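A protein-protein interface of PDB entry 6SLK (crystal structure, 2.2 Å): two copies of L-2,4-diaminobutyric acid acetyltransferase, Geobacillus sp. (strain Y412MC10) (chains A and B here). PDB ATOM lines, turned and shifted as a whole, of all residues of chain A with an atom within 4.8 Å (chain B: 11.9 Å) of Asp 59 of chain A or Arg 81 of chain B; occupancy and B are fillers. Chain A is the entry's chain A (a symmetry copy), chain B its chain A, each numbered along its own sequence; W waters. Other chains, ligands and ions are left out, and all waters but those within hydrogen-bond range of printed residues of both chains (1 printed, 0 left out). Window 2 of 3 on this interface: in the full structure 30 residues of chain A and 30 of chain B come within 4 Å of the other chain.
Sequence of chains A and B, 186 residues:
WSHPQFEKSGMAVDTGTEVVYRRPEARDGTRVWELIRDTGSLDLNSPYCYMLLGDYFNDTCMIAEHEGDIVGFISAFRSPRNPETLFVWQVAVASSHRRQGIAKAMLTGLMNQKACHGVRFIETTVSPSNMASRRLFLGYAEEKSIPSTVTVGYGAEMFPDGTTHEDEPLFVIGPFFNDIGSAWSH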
ATOM      1  N   ARG A  23     -32.158  10.273 -22.398  1.00  0.00           N
ATOM      2  CA  ARG A  23     -32.267   8.832 -22.290  1.00  0.00           C
ATOM      3  C   ARG A  23     -33.473   8.453 -21.473  1.00  0.00           C
ATOM      4  O   ARG A  23     -33.849   9.142 -20.543  1.00  0.00           O
ATOM      5  CB  ARG A  23     -31.015   8.209 -21.713  1.00  0.00           C
ATOM      6  CG  ARG A  23     -29.849   8.264 -22.691  1.00  0.00           C
ATOM      7  CD  ARG A  23     -28.630   7.518 -22.178  1.00  0.00           C
ATOM      8  NE  ARG A  23     -28.149   8.152 -20.953  1.00  0.00           N
ATOM      9  CZ  ARG A  23     -27.203   9.092 -20.872  1.00  0.00           C
ATOM     10  NH1 ARG A  23     -26.510   9.543 -21.921  1.00  0.00           N
ATOM     11  NH2 ARG A  23     -26.923   9.584 -19.689  1.00  0.00           N
ATOM     12  N   ASP A  55     -34.500   0.007 -19.900  1.00  0.00           N
ATOM     13  CA  ASP A  55     -33.628  -0.529 -18.905  1.00  0.00           C
ATOM     14  C   ASP A  55     -32.324  -0.888 -19.593  1.00  0.00           C
ATOM     15  O   ASP A  55     -31.327  -0.277 -19.291  1.00  0.00           O
ATOM     16  CB  ASP A  55     -34.357  -1.753 -18.328  1.00  0.00           C
ATOM     17  CG  ASP A  55     -33.811  -2.212 -16.995  1.00  0.00           C
ATOM     18  OD1 ASP A  55     -32.706  -1.808 -16.683  1.00  0.00           O
ATOM     19  OD2 ASP A  55     -34.484  -3.042 -16.313  1.00  0.00           O
ATOM     20  N   TYR A  56     -32.330  -1.862 -20.525  1.00  0.00           N
ATOM     21  CA  TYR A  56     -31.104  -2.472 -21.017  1.00  0.00           C
ATOM     22  C   TYR A  56     -30.510  -1.715 -22.233  1.00  0.00           C
ATOM     23  O   TYR A  56     -29.274  -1.758 -22.467  1.00  0.00           O
ATOM     24  CB  TYR A  56     -31.332  -3.955 -21.331  1.00  0.00           C
ATOM     25  CG  TYR A  56     -31.590  -4.784 -20.047  1.00  0.00           C
ATOM     26  CD1 TYR A  56     -30.520  -5.276 -19.269  1.00  0.00           C
ATOM     27  CD2 TYR A  56     -32.876  -5.082 -19.622  1.00  0.00           C
ATOM     28  CE1 TYR A  56     -30.742  -6.063 -18.112  1.00  0.00           C
ATOM     29  CE2 TYR A  56     -33.122  -5.830 -18.450  1.00  0.00           C
ATOM     30  CZ  TYR A  56     -32.050  -6.295 -17.682  1.00  0.00           C
ATOM     31  OH  TYR A  56     -32.234  -6.982 -16.525  1.00  0.00           O
ATOM     32  N   PHE A  57     -31.349  -0.999 -22.965  1.00  0.00           N
ATOM     33  CA  PHE A  57     -30.895  -0.367 -24.215  1.00  0.00           C
ATOM     34  C   PHE A  57     -30.841   1.176 -24.173  1.00  0.00           C
ATOM     35  O   PHE A  57     -30.617   1.845 -25.201  1.00  0.00           O
ATOM     36  CB  PHE A  57     -31.806  -0.851 -25.339  1.00  0.00           C
ATOM     37  CG  PHE A  57     -31.601  -2.298 -25.682  1.00  0.00           C
ATOM     38  CD1 PHE A  57     -30.555  -2.675 -26.486  1.00  0.00           C
ATOM     39  CD2 PHE A  57     -32.453  -3.287 -25.195  1.00  0.00           C
ATOM     40  CE1 PHE A  57     -30.337  -4.031 -26.812  1.00  0.00           C
ATOM     41  CE2 PHE A  57     -32.250  -4.645 -25.492  1.00  0.00           C
ATOM     42  CZ  PHE A  57     -31.206  -5.016 -26.314  1.00  0.00           C
ATOM     43  N   ASN A  58     -30.990   1.755 -22.988  1.00  0.00           N
ATOM     44  CA  ASN A  58     -31.267   3.167 -22.925  1.00  0.00           C
ATOM     45  C   ASN A  58     -30.098   4.059 -23.303  1.00  0.00           C
ATOM     46  O   ASN A  58     -30.281   5.172 -23.710  1.00  0.00           O
ATOM     47  CB  ASN A  58     -31.950   3.530 -21.604  1.00  0.00           C
ATOM     48  CG  ASN A  58     -30.992   3.648 -20.411  1.00  0.00           C
ATOM     49  OD1 ASN A  58     -29.880   3.134 -20.374  1.00  0.00           O
ATOM     50  ND2 ASN A  58     -31.431   4.421 -19.448  1.00  0.00           N
ATOM     51  N   ASP A  59     -28.905   3.515 -23.327  1.00  0.00           N
ATOM     52  CA  ASP A  59     -27.788   4.248 -23.822  1.00  0.00           C
ATOM     53  C   ASP A  59     -27.833   4.647 -25.318  1.00  0.00           C
ATOM     54  O   ASP A  59     -27.044   5.527 -25.741  1.00  0.00           O
ATOM     55  CB  ASP A  59     -26.492   3.433 -23.598  1.00  0.00           C
ATOM     56  CG  ASP A  59     -26.310   3.039 -22.123  1.00  0.00           C
ATOM     57  OD1 ASP A  59     -25.807   3.865 -21.395  1.00  0.00           O
ATOM     58  OD2 ASP A  59     -26.743   1.948 -21.695  1.00  0.00           O
ATOM     59  N   THR A  60     -28.608   3.894 -26.094  1.00  0.00           N
ATOM     60  CA  THR A  60     -28.775   4.095 -27.532  1.00  0.00           C
ATOM     61  C   THR A  60     -30.239   4.310 -27.855  1.00  0.00           C
ATOM     62  O   THR A  60     -30.647   3.932 -28.935  1.00  0.00           O
ATOM     63  CB  THR A  60     -28.289   2.862 -28.321  1.00  0.00           C
ATOM     64  OG1 THR A  60     -28.959   1.668 -27.895  1.00  0.00           O
ATOM     65  CG2 THR A  60     -26.875   2.695 -28.151  1.00  0.00           C
ATOM     66  N   CYS A  61     -31.034   4.842 -26.905  1.00  0.00           N
ATOM     67  CA  CYS A  61     -32.443   5.279 -27.139  1.00  0.00           C
ATOM     68  C   CYS A  61     -32.578   6.739 -26.714  1.00  0.00           C
ATOM     69  O   CYS A  61     -31.679   7.269 -26.027  1.00  0.00           O
ATOM     70  CB  CYS A  61     -33.493   4.472 -26.361  1.00  0.00           C
ATOM     71  SG  CYS A  61     -33.483   2.707 -26.847  1.00  0.00           S
ATOM     72  N   GLN A 113     -24.697  10.766 -28.459  1.00  0.00           N
ATOM     73  CA  GLN A 113     -24.496   9.997 -27.237  1.00  0.00           C
ATOM     74  C   GLN A 113     -23.170   9.264 -27.146  1.00  0.00           C
ATOM     75  O   GLN A 113     -22.676   8.701 -28.127  1.00  0.00           O
ATOM     76  CB  GLN A 113     -25.569   8.916 -27.113  1.00  0.00           C
ATOM     77  CG  GLN A 113     -26.995   9.399 -27.007  1.00  0.00           C
ATOM     78  CD  GLN A 113     -27.283  10.158 -25.734  1.00  0.00           C
ATOM     79  OE1 GLN A 113     -26.496  10.983 -25.291  1.00  0.00           O
ATOM     80  NE2 GLN A 113     -28.444   9.914 -25.176  1.00  0.00           N
ATOM     81  N   ALA A 115     -22.557   6.363 -26.033  1.00  0.00           N
ATOM     82  CA  ALA A 115     -22.635   4.965 -26.474  1.00  0.00           C
ATOM     83  C   ALA A 115     -22.627   4.769 -28.013  1.00  0.00           C
ATOM     84  O   ALA A 115     -22.529   3.624 -28.452  1.00  0.00           O
ATOM     85  CB  ALA A 115     -23.831   4.285 -25.860  1.00  0.00           C
ATOM     86  N   PHE B  57     -30.381 -10.719 -33.584  1.00  0.00           N
ATOM     87  CA  PHE B  57     -30.096 -11.338 -32.278  1.00  0.00           C
ATOM     88  C   PHE B  57     -29.982 -12.878 -32.308  1.00  0.00           C
ATOM     89  O   PHE B  57     -29.891 -13.542 -31.256  1.00  0.00           O
ATOM     90  CB  PHE B  57     -31.181 -10.889 -31.304  1.00  0.00           C
ATOM     91  CG  PHE B  57     -31.080  -9.437 -30.938  1.00  0.00           C
ATOM     92  CD1 PHE B  57     -30.180  -9.026 -29.988  1.00  0.00           C
ATOM     93  CD2 PHE B  57     -31.884  -8.477 -31.549  1.00  0.00           C
ATOM     94  CE1 PHE B  57     -30.060  -7.663 -29.637  1.00  0.00           C
ATOM     95  CE2 PHE B  57     -31.776  -7.114 -31.228  1.00  0.00           C
ATOM     96  CZ  PHE B  57     -30.880  -6.708 -30.261  1.00  0.00           C
ATOM     97  N   PHE B  77     -30.497 -11.696 -25.221  1.00  0.00           N
ATOM     98  CA  PHE B  77     -29.412 -10.842 -25.683  1.00  0.00           C
ATOM     99  C   PHE B  77     -28.415 -10.612 -24.602  1.00  0.00           C
ATOM    100  O   PHE B  77     -28.758 -10.660 -23.464  1.00  0.00           O
ATOM    101  CB  PHE B  77     -29.957  -9.468 -26.131  1.00  0.00           C
ATOM    102  CG  PHE B  77     -30.822  -8.768 -25.101  1.00  0.00           C
ATOM    103  CD1 PHE B  77     -30.255  -7.929 -24.142  1.00  0.00           C
ATOM    104  CD2 PHE B  77     -32.170  -8.937 -25.102  1.00  0.00           C
ATOM    105  CE1 PHE B  77     -31.037  -7.293 -23.184  1.00  0.00           C
ATOM    106  CE2 PHE B  77     -32.949  -8.294 -24.161  1.00  0.00           C
ATOM    107  CZ  PHE B  77     -32.388  -7.469 -23.208  1.00  0.00           C
ATOM    108  N   ARG B  78     -27.206 -10.274 -24.982  1.00  0.00           N
ATOM    109  CA  ARG B  78     -26.236  -9.838 -24.020  1.00  0.00           C
ATOM    110  C   ARG B  78     -26.422  -8.384 -23.702  1.00  0.00           C
ATOM    111  O   ARG B  78     -26.563  -7.533 -24.589  1.00  0.00           O
ATOM    112  CB  ARG B  78     -24.803 -10.117 -24.491  1.00  0.00           C
ATOM    113  CG  ARG B  78     -24.673 -11.580 -24.814  1.00  0.00           C
ATOM    114  CD  ARG B  78     -23.285 -12.029 -25.277  1.00  0.00           C
ATOM    115  NE  ARG B  78     -22.245 -11.838 -24.277  1.00  0.00           N
ATOM    116  CZ  ARG B  78     -21.104 -12.501 -24.258  1.00  0.00           C
ATOM    117  NH1 ARG B  78     -20.852 -13.486 -25.125  1.00  0.00           N
ATOM    118  NH2 ARG B  78     -20.238 -12.222 -23.314  1.00  0.00           N
ATOM    119  N   SER B  79     -26.438  -8.077 -22.411  1.00  0.00           N
ATOM    120  CA  SER B  79     -26.655  -6.726 -21.979  1.00  0.00           C
ATOM    121  C   SER B  79     -25.583  -5.728 -22.548  1.00  0.00           C
ATOM    122  O   SER B  79     -24.347  -5.881 -22.317  1.00  0.00           O
ATOM    123  CB  SER B  79     -26.673  -6.658 -20.460  1.00  0.00           C
ATOM    124  OG  SER B  79     -26.692  -5.303 -20.062  1.00  0.00           O
ATOM    125  N   PRO B  80     -26.041  -4.688 -23.266  1.00  0.00           N
ATOM    126  CA  PRO B  80     -25.037  -3.776 -23.840  1.00  0.00           C
ATOM    127  C   PRO B  80     -24.062  -3.081 -22.864  1.00  0.00           C
ATOM    128  O   PRO B  80     -22.869  -3.024 -23.140  1.00  0.00           O
ATOM    129  CB  PRO B  80     -25.915  -2.730 -24.599  1.00  0.00           C
ATOM    130  CG  PRO B  80     -27.117  -3.531 -25.020  1.00  0.00           C
ATOM    131  CD  PRO B  80     -27.382  -4.465 -23.851  1.00  0.00           C
ATOM    132  N   ARG B  81     -24.577  -2.574 -21.745  1.00  0.00           N
ATOM    133  CA  ARG B  81     -23.735  -2.094 -20.628  1.00  0.00           C
ATOM    134  C   ARG B  81     -22.880  -3.144 -19.942  1.00  0.00           C
ATOM    135  O   ARG B  81     -21.820  -2.797 -19.487  1.00  0.00           O
ATOM    136  CB  ARG B  81     -24.584  -1.404 -19.519  1.00  0.00           C
ATOM    137  CG  ARG B  81     -25.254  -0.124 -20.017  1.00  0.00           C
ATOM    138  CD  ARG B  81     -25.745   0.791 -18.876  1.00  0.00           C
ATOM    139  NE  ARG B  81     -26.803   0.067 -18.257  1.00  0.00           N
ATOM    140  CZ  ARG B  81     -28.054  -0.026 -18.695  1.00  0.00           C
ATOM    141  NH1 ARG B  81     -28.510   0.654 -19.777  1.00  0.00           N
ATOM    142  NH2 ARG B  81     -28.881  -0.807 -18.008  1.00  0.00           N
ATOM    143  N   ASN B  82     -23.285  -4.415 -19.895  1.00  0.00           N
ATOM    144  CA  ASN B  82     -22.615  -5.470 -19.090  1.00  0.00           C
ATOM    145  C   ASN B  82     -22.685  -6.737 -19.873  1.00  0.00           C
ATOM    146  O   ASN B  82     -23.532  -7.610 -19.614  1.00  0.00           O
ATOM    147  CB  ASN B  82     -23.371  -5.657 -17.746  1.00  0.00           C
ATOM    148  CG  ASN B  82     -23.312  -4.397 -16.886  1.00  0.00           C
ATOM    149  OD1 ASN B  82     -22.231  -3.948 -16.525  1.00  0.00           O
ATOM    150  ND2 ASN B  82     -24.474  -3.775 -16.609  1.00  0.00           N
ATOM    151  N   PRO B  83     -21.874  -6.815 -20.930  1.00  0.00           N
ATOM    152  CA  PRO B  83     -21.950  -7.929 -21.877  1.00  0.00           C
ATOM    153  C   PRO B  83     -21.610  -9.292 -21.315  1.00  0.00           C
ATOM    154  O   PRO B  83     -21.867 -10.257 -22.018  1.00  0.00           O
ATOM    155  CB  PRO B  83     -20.908  -7.587 -22.944  1.00  0.00           C
ATOM    156  CG  PRO B  83     -20.459  -6.216 -22.652  1.00  0.00           C
ATOM    157  CD  PRO B  83     -20.838  -5.828 -21.284  1.00  0.00           C
ATOM    158  N   GLU B  84     -21.043  -9.366 -20.110  1.00  0.00           N
ATOM    159  CA  GLU B  84     -20.911 -10.660 -19.370  1.00  0.00           C
ATOM    160  C   GLU B  84     -22.234 -11.217 -18.830  1.00  0.00           C
ATOM    161  O   GLU B  84     -22.281 -12.333 -18.347  1.00  0.00           O
ATOM    162  CB  GLU B  84     -19.806 -10.583 -18.265  1.00  0.00           C
ATOM    163  CG  GLU B  84     -18.391 -10.297 -18.854  1.00  0.00           C
ATOM    164  CD  GLU B  84     -17.212 -10.186 -17.842  1.00  0.00           C
ATOM    165  OE1 GLU B  84     -17.445  -9.750 -16.689  1.00  0.00           O
ATOM    166  OE2 GLU B  84     -16.035 -10.510 -18.207  1.00  0.00           O
ATOM    167  N   THR B  85     -23.307 -10.440 -18.929  1.00  0.00           N
ATOM    168  CA  THR B  85     -24.661 -10.873 -18.545  1.00  0.00           C
ATOM    169  C   THR B  85     -25.525 -11.135 -19.762  1.00  0.00           C
ATOM    170  O   THR B  85     -25.680 -10.262 -20.631  1.00  0.00           O
ATOM    171  CB  THR B  85     -25.342  -9.799 -17.673  1.00  0.00           C
ATOM    172  OG1 THR B  85     -24.689  -9.755 -16.388  1.00  0.00           O
ATOM    173  CG2 THR B  85     -26.837 -10.076 -17.510  1.00  0.00           C
ATOM    174  N   LEU B  86     -26.094 -12.323 -19.822  1.00  0.00           N
ATOM    175  CA  LEU B  86     -27.106 -12.644 -20.789  1.00  0.00           C
ATOM    176  C   LEU B  86     -28.471 -12.469 -20.164  1.00  0.00           C
ATOM    177  O   LEU B  86     -28.798 -13.098 -19.140  1.00  0.00           O
ATOM    178  CB  LEU B  86     -26.944 -14.091 -21.236  1.00  0.00           C
ATOM    179  CG  LEU B  86     -27.918 -14.605 -22.302  1.00  0.00           C
ATOM    180  CD1 LEU B  86     -27.526 -14.015 -23.677  1.00  0.00           C
ATOM    181  CD2 LEU B  86     -28.013 -16.095 -22.418  1.00  0.00           C
ATOM    182  N   PHE B  87     -29.289 -11.655 -20.797  1.00  0.00           N
ATOM    183  CA  PHE B  87     -30.647 -11.495 -20.433  1.00  0.00           C
ATOM    184  C   PHE B  87     -31.540 -12.366 -21.287  1.00  0.00           C
ATOM    185  O   PHE B  87     -31.523 -12.252 -22.501  1.00  0.00           O
ATOM    186  CB  PHE B  87     -31.076 -10.024 -20.617  1.00  0.00           C
ATOM    187  CG  PHE B  87     -32.445  -9.763 -20.112  1.00  0.00           C
ATOM    188  CD1 PHE B  87     -32.633  -9.433 -18.773  1.00  0.00           C
ATOM    189  CD2 PHE B  87     -33.520  -9.931 -20.903  1.00  0.00           C
ATOM    190  CE1 PHE B  87     -33.899  -9.231 -18.253  1.00  0.00           C
ATOM    191  CE2 PHE B  87     -34.820  -9.684 -20.415  1.00  0.00           C
ATOM    192  CZ  PHE B  87     -35.010  -9.357 -19.083  1.00  0.00           C
ATOM    193  N   GLY B 118     -17.863 -16.363 -22.555  1.00  0.00           N
ATOM    194  CA  GLY B 118     -17.570 -15.319 -21.612  1.00  0.00           C
ATOM    195  C   GLY B 118     -18.704 -14.805 -20.742  1.00  0.00           C
ATOM    196  O   GLY B 118     -18.504 -13.857 -19.963  1.00  0.00           O
ATOM    197  N   VAL B 119     -19.887 -15.378 -20.892  1.00  0.00           N
ATOM    198  CA  VAL B 119     -21.016 -15.001 -20.020  1.00  0.00           C
ATOM    199  C   VAL B 119     -20.771 -15.587 -18.607  1.00  0.00           C
ATOM    200  O   VAL B 119     -20.381 -16.721 -18.461  1.00  0.00           O
ATOM    201  CB  VAL B 119     -22.365 -15.530 -20.571  1.00  0.00           C
ATOM    202  CG1 VAL B 119     -23.482 -15.279 -19.562  1.00  0.00           C
ATOM    203  CG2 VAL B 119     -22.705 -14.833 -21.920  1.00  0.00           C
ATOM    204  N   PHE B 121     -23.222 -14.327 -15.928  1.00  0.00           N
ATOM    205  CA  PHE B 121     -24.570 -14.287 -15.315  1.00  0.00           C
ATOM    206  C   PHE B 121     -25.668 -14.472 -16.365  1.00  0.00           C
ATOM    207  O   PHE B 121     -25.496 -14.048 -17.529  1.00  0.00           O
ATOM    208  CB  PHE B 121     -24.852 -12.995 -14.641  1.00  0.00           C
ATOM    209  CG  PHE B 121     -23.955 -12.677 -13.522  1.00  0.00           C
ATOM    210  CD1 PHE B 121     -24.214 -13.172 -12.258  1.00  0.00           C
ATOM    211  CD2 PHE B 121     -22.839 -11.825 -13.709  1.00  0.00           C
ATOM    212  CE1 PHE B 121     -23.397 -12.824 -11.180  1.00  0.00           C
ATOM    213  CE2 PHE B 121     -22.007 -11.494 -12.640  1.00  0.00           C
ATOM    214  CZ  PHE B 121     -22.301 -11.992 -11.365  1.00  0.00           C
ATOM    215  N   GLU B 123     -29.730 -13.304 -16.455  1.00  0.00           N
ATOM    216  CA  GLU B 123     -30.675 -12.422 -15.809  1.00  0.00           C
ATOM    217  C   GLU B 123     -31.973 -12.573 -16.599  1.00  0.00           C
ATOM    218  O   GLU B 123     -31.962 -12.809 -17.839  1.00  0.00           O
ATOM    219  CB  GLU B 123     -30.073 -11.071 -15.838  1.00  0.00           C
ATOM    220  CG  GLU B 123     -30.747 -10.050 -15.061  1.00  0.00           C
ATOM    221  CD  GLU B 123     -29.827  -8.869 -14.854  1.00  0.00           C
ATOM    222  OE1 GLU B 123     -28.730  -9.022 -14.282  1.00  0.00           O
ATOM    223  OE2 GLU B 123     -30.214  -7.767 -15.293  1.00  0.00           O
ATOM    224  N   TYR B 154     -39.701  -5.609 -11.819  1.00  0.00           N
ATOM    225  CA  TYR B 154     -40.654  -4.556 -12.201  1.00  0.00           C
ATOM    226  C   TYR B 154     -41.932  -4.864 -11.416  1.00  0.00           C
ATOM    227  O   TYR B 154     -42.347  -6.029 -11.305  1.00  0.00           O
ATOM    228  CB  TYR B 154     -40.940  -4.498 -13.749  1.00  0.00           C
ATOM    229  CG  TYR B 154     -39.724  -4.403 -14.668  1.00  0.00           C
ATOM    230  CD1 TYR B 154     -38.710  -3.466 -14.444  1.00  0.00           C
ATOM    231  CD2 TYR B 154     -39.589  -5.247 -15.779  1.00  0.00           C
ATOM    232  CE1 TYR B 154     -37.565  -3.453 -15.243  1.00  0.00           C
ATOM    233  CE2 TYR B 154     -38.458  -5.198 -16.615  1.00  0.00           C
ATOM    234  CZ  TYR B 154     -37.469  -4.303 -16.362  1.00  0.00           C
ATOM    235  OH  TYR B 154     -36.327  -4.305 -17.154  1.00  0.00           O
ATOM    236  N   LEU B 170     -37.046 -10.224 -10.580  1.00  0.00           N
ATOM    237  CA  LEU B 170     -35.775 -10.468 -11.220  1.00  0.00           C
ATOM    238  C   LEU B 170     -35.050 -11.696 -10.695  1.00  0.00           C
ATOM    239  O   LEU B 170     -34.934 -11.897  -9.478  1.00  0.00           O
ATOM    240  CB  LEU B 170     -34.925  -9.228 -10.979  1.00  0.00           C
ATOM    241  CG  LEU B 170     -33.605  -9.166 -11.736  1.00  0.00           C
ATOM    242  CD1 LEU B 170     -33.834  -8.976 -13.222  1.00  0.00           C
ATOM    243  CD2 LEU B 170     -32.682  -8.108 -11.154  1.00  0.00           C
HETATM  244  O   HOH W   1     -27.321  -2.883 -20.830  1.00  0.00           O
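OD2 of Asp 55 of chain A lies close to OH of Tyr 154 of chain B (2.4 Å). The guanidinium group of Arg 81 of chain B lies within hydrogen-bond range of the backbone carbonyl oxygen of Asp 55 of chain A, 2.8 Å away. The side-chain carboxylate (OE2) of Glu 123 of chain B is in hydrogen-bond range of the side-chain hydroxyl (OH) of Tyr 56 of chain A (2.5 Å). NH1 of Arg 81 of chain B is in salt-bridge range of OD2 of Asp 59 of chain A. OD1 of Asn 58 of chain A lies within hydrogen-bond range of NH1 of Arg 81 of chain B (2.9 Å).
The backbone NH of Ser 79 of chain B is in hydrogen-bond range of the backbone carbonyl oxygen of Thr 85 of chain B, at 2.9 Å. The side-chain hydroxyl (OG1) of Thr 60 of chain A lies within hydrogen-bond range of the backbone carbonyl oxygen (O) of Phe 57 of chain A (3.2 Å). O of Phe 57 of chain A is in hydrogen-bond range of SG of Cys 61 of chain A (3.4 Å). The backbone carbonyl oxygen of Leu 86 of chain B sits at hydrogen-bond distance from the backbone NH of Glu 123 of chain B (2.8 Å). The backbone carbonyl oxygen of Phe 77 of chain B is in hydrogen-bond range of the backbone NH of Phe 87 of chain B.
Tyr 56 of chain A touches Phe 77 of chain B. Ser 79 of chain B touches Tyr 56 of chain A. Pro 80 of chain B touches Tyr 56 of chain A. Arg 81 of chain B touches Tyr 56 of chain A (NH1 to O, 3.7 Å). Phe 87 of chain B touches Tyr 56 of chain A (CE1 to OH, 3.3 Å). Tyr 154 of chain B touches Tyr 56 of chain A. Phe 57 of chain A touches Phe 77 of chain B. CE1 of Phe 57 of chain A touches CG of Pro 80 of chain B, 3.7 Å away.
Asp 55 of chain A touches just these residues of chain B: Arg 81 (2.8 Å) and Tyr 154 (2.4 Å). Printed residues of chain B within 4 Å of Tyr 56 of chain A: Phe 77 (3.8 Å), Ser 79 (3.9 Å), Pro 80 (3.6 Å), Arg 81 (3.7 Å), Phe 87 (3.3 Å), Glu 123 (2.5 Å) and Tyr 154 (3.8 Å). Of chain B, only Arg 81 comes within 4 Å of Asp 59 of chain A. No residue of chain B comes within 4 Å of Thr 60 of chain A. No residue of chain B comes within 4 Å of Cys 61 of chain A. No residue of chain B comes within 4 Å of Gln 113 of chain A. No residue of chain B comes within 4 Å of Ala 115 of chain A. Of the printed residues of chain A, Ser 79 of chain B touches Tyr 56. Of the printed residues of chain A, Phe 87 of chain B touches Tyr 56 (3.3 Å). Gly 118 of chain B touches none of the printed residues of chain A. The nearest residue of chain A that does not touch Arg 81 of chain B is Phe 57 of chain A (4.6 Å). The nearest printed residue of chain A that does not touch Phe 87 of chain B is Asp 55 of chain A (6.5 Å).
Hydrophobic or aromatic side chains of chain B within 4 Å of the printed part of chain A: Phe 77, Pro 80, Phe 87 and Tyr 154. Hydrophobic or aromatic side chains of chain A within 4 Å of the printed part of chain B: Tyr 56 and Phe 57.
1 position is printed for both chains.
Water W1 lies within hydrogen-bond range of the side-chain hydroxyl of Ser 79 of chain B (2.6 Å), the backbone carbonyl oxygen of Tyr 56 of chain A (2.8 Å) and the backbone NH of Arg 81 of chain B (2.9 Å).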
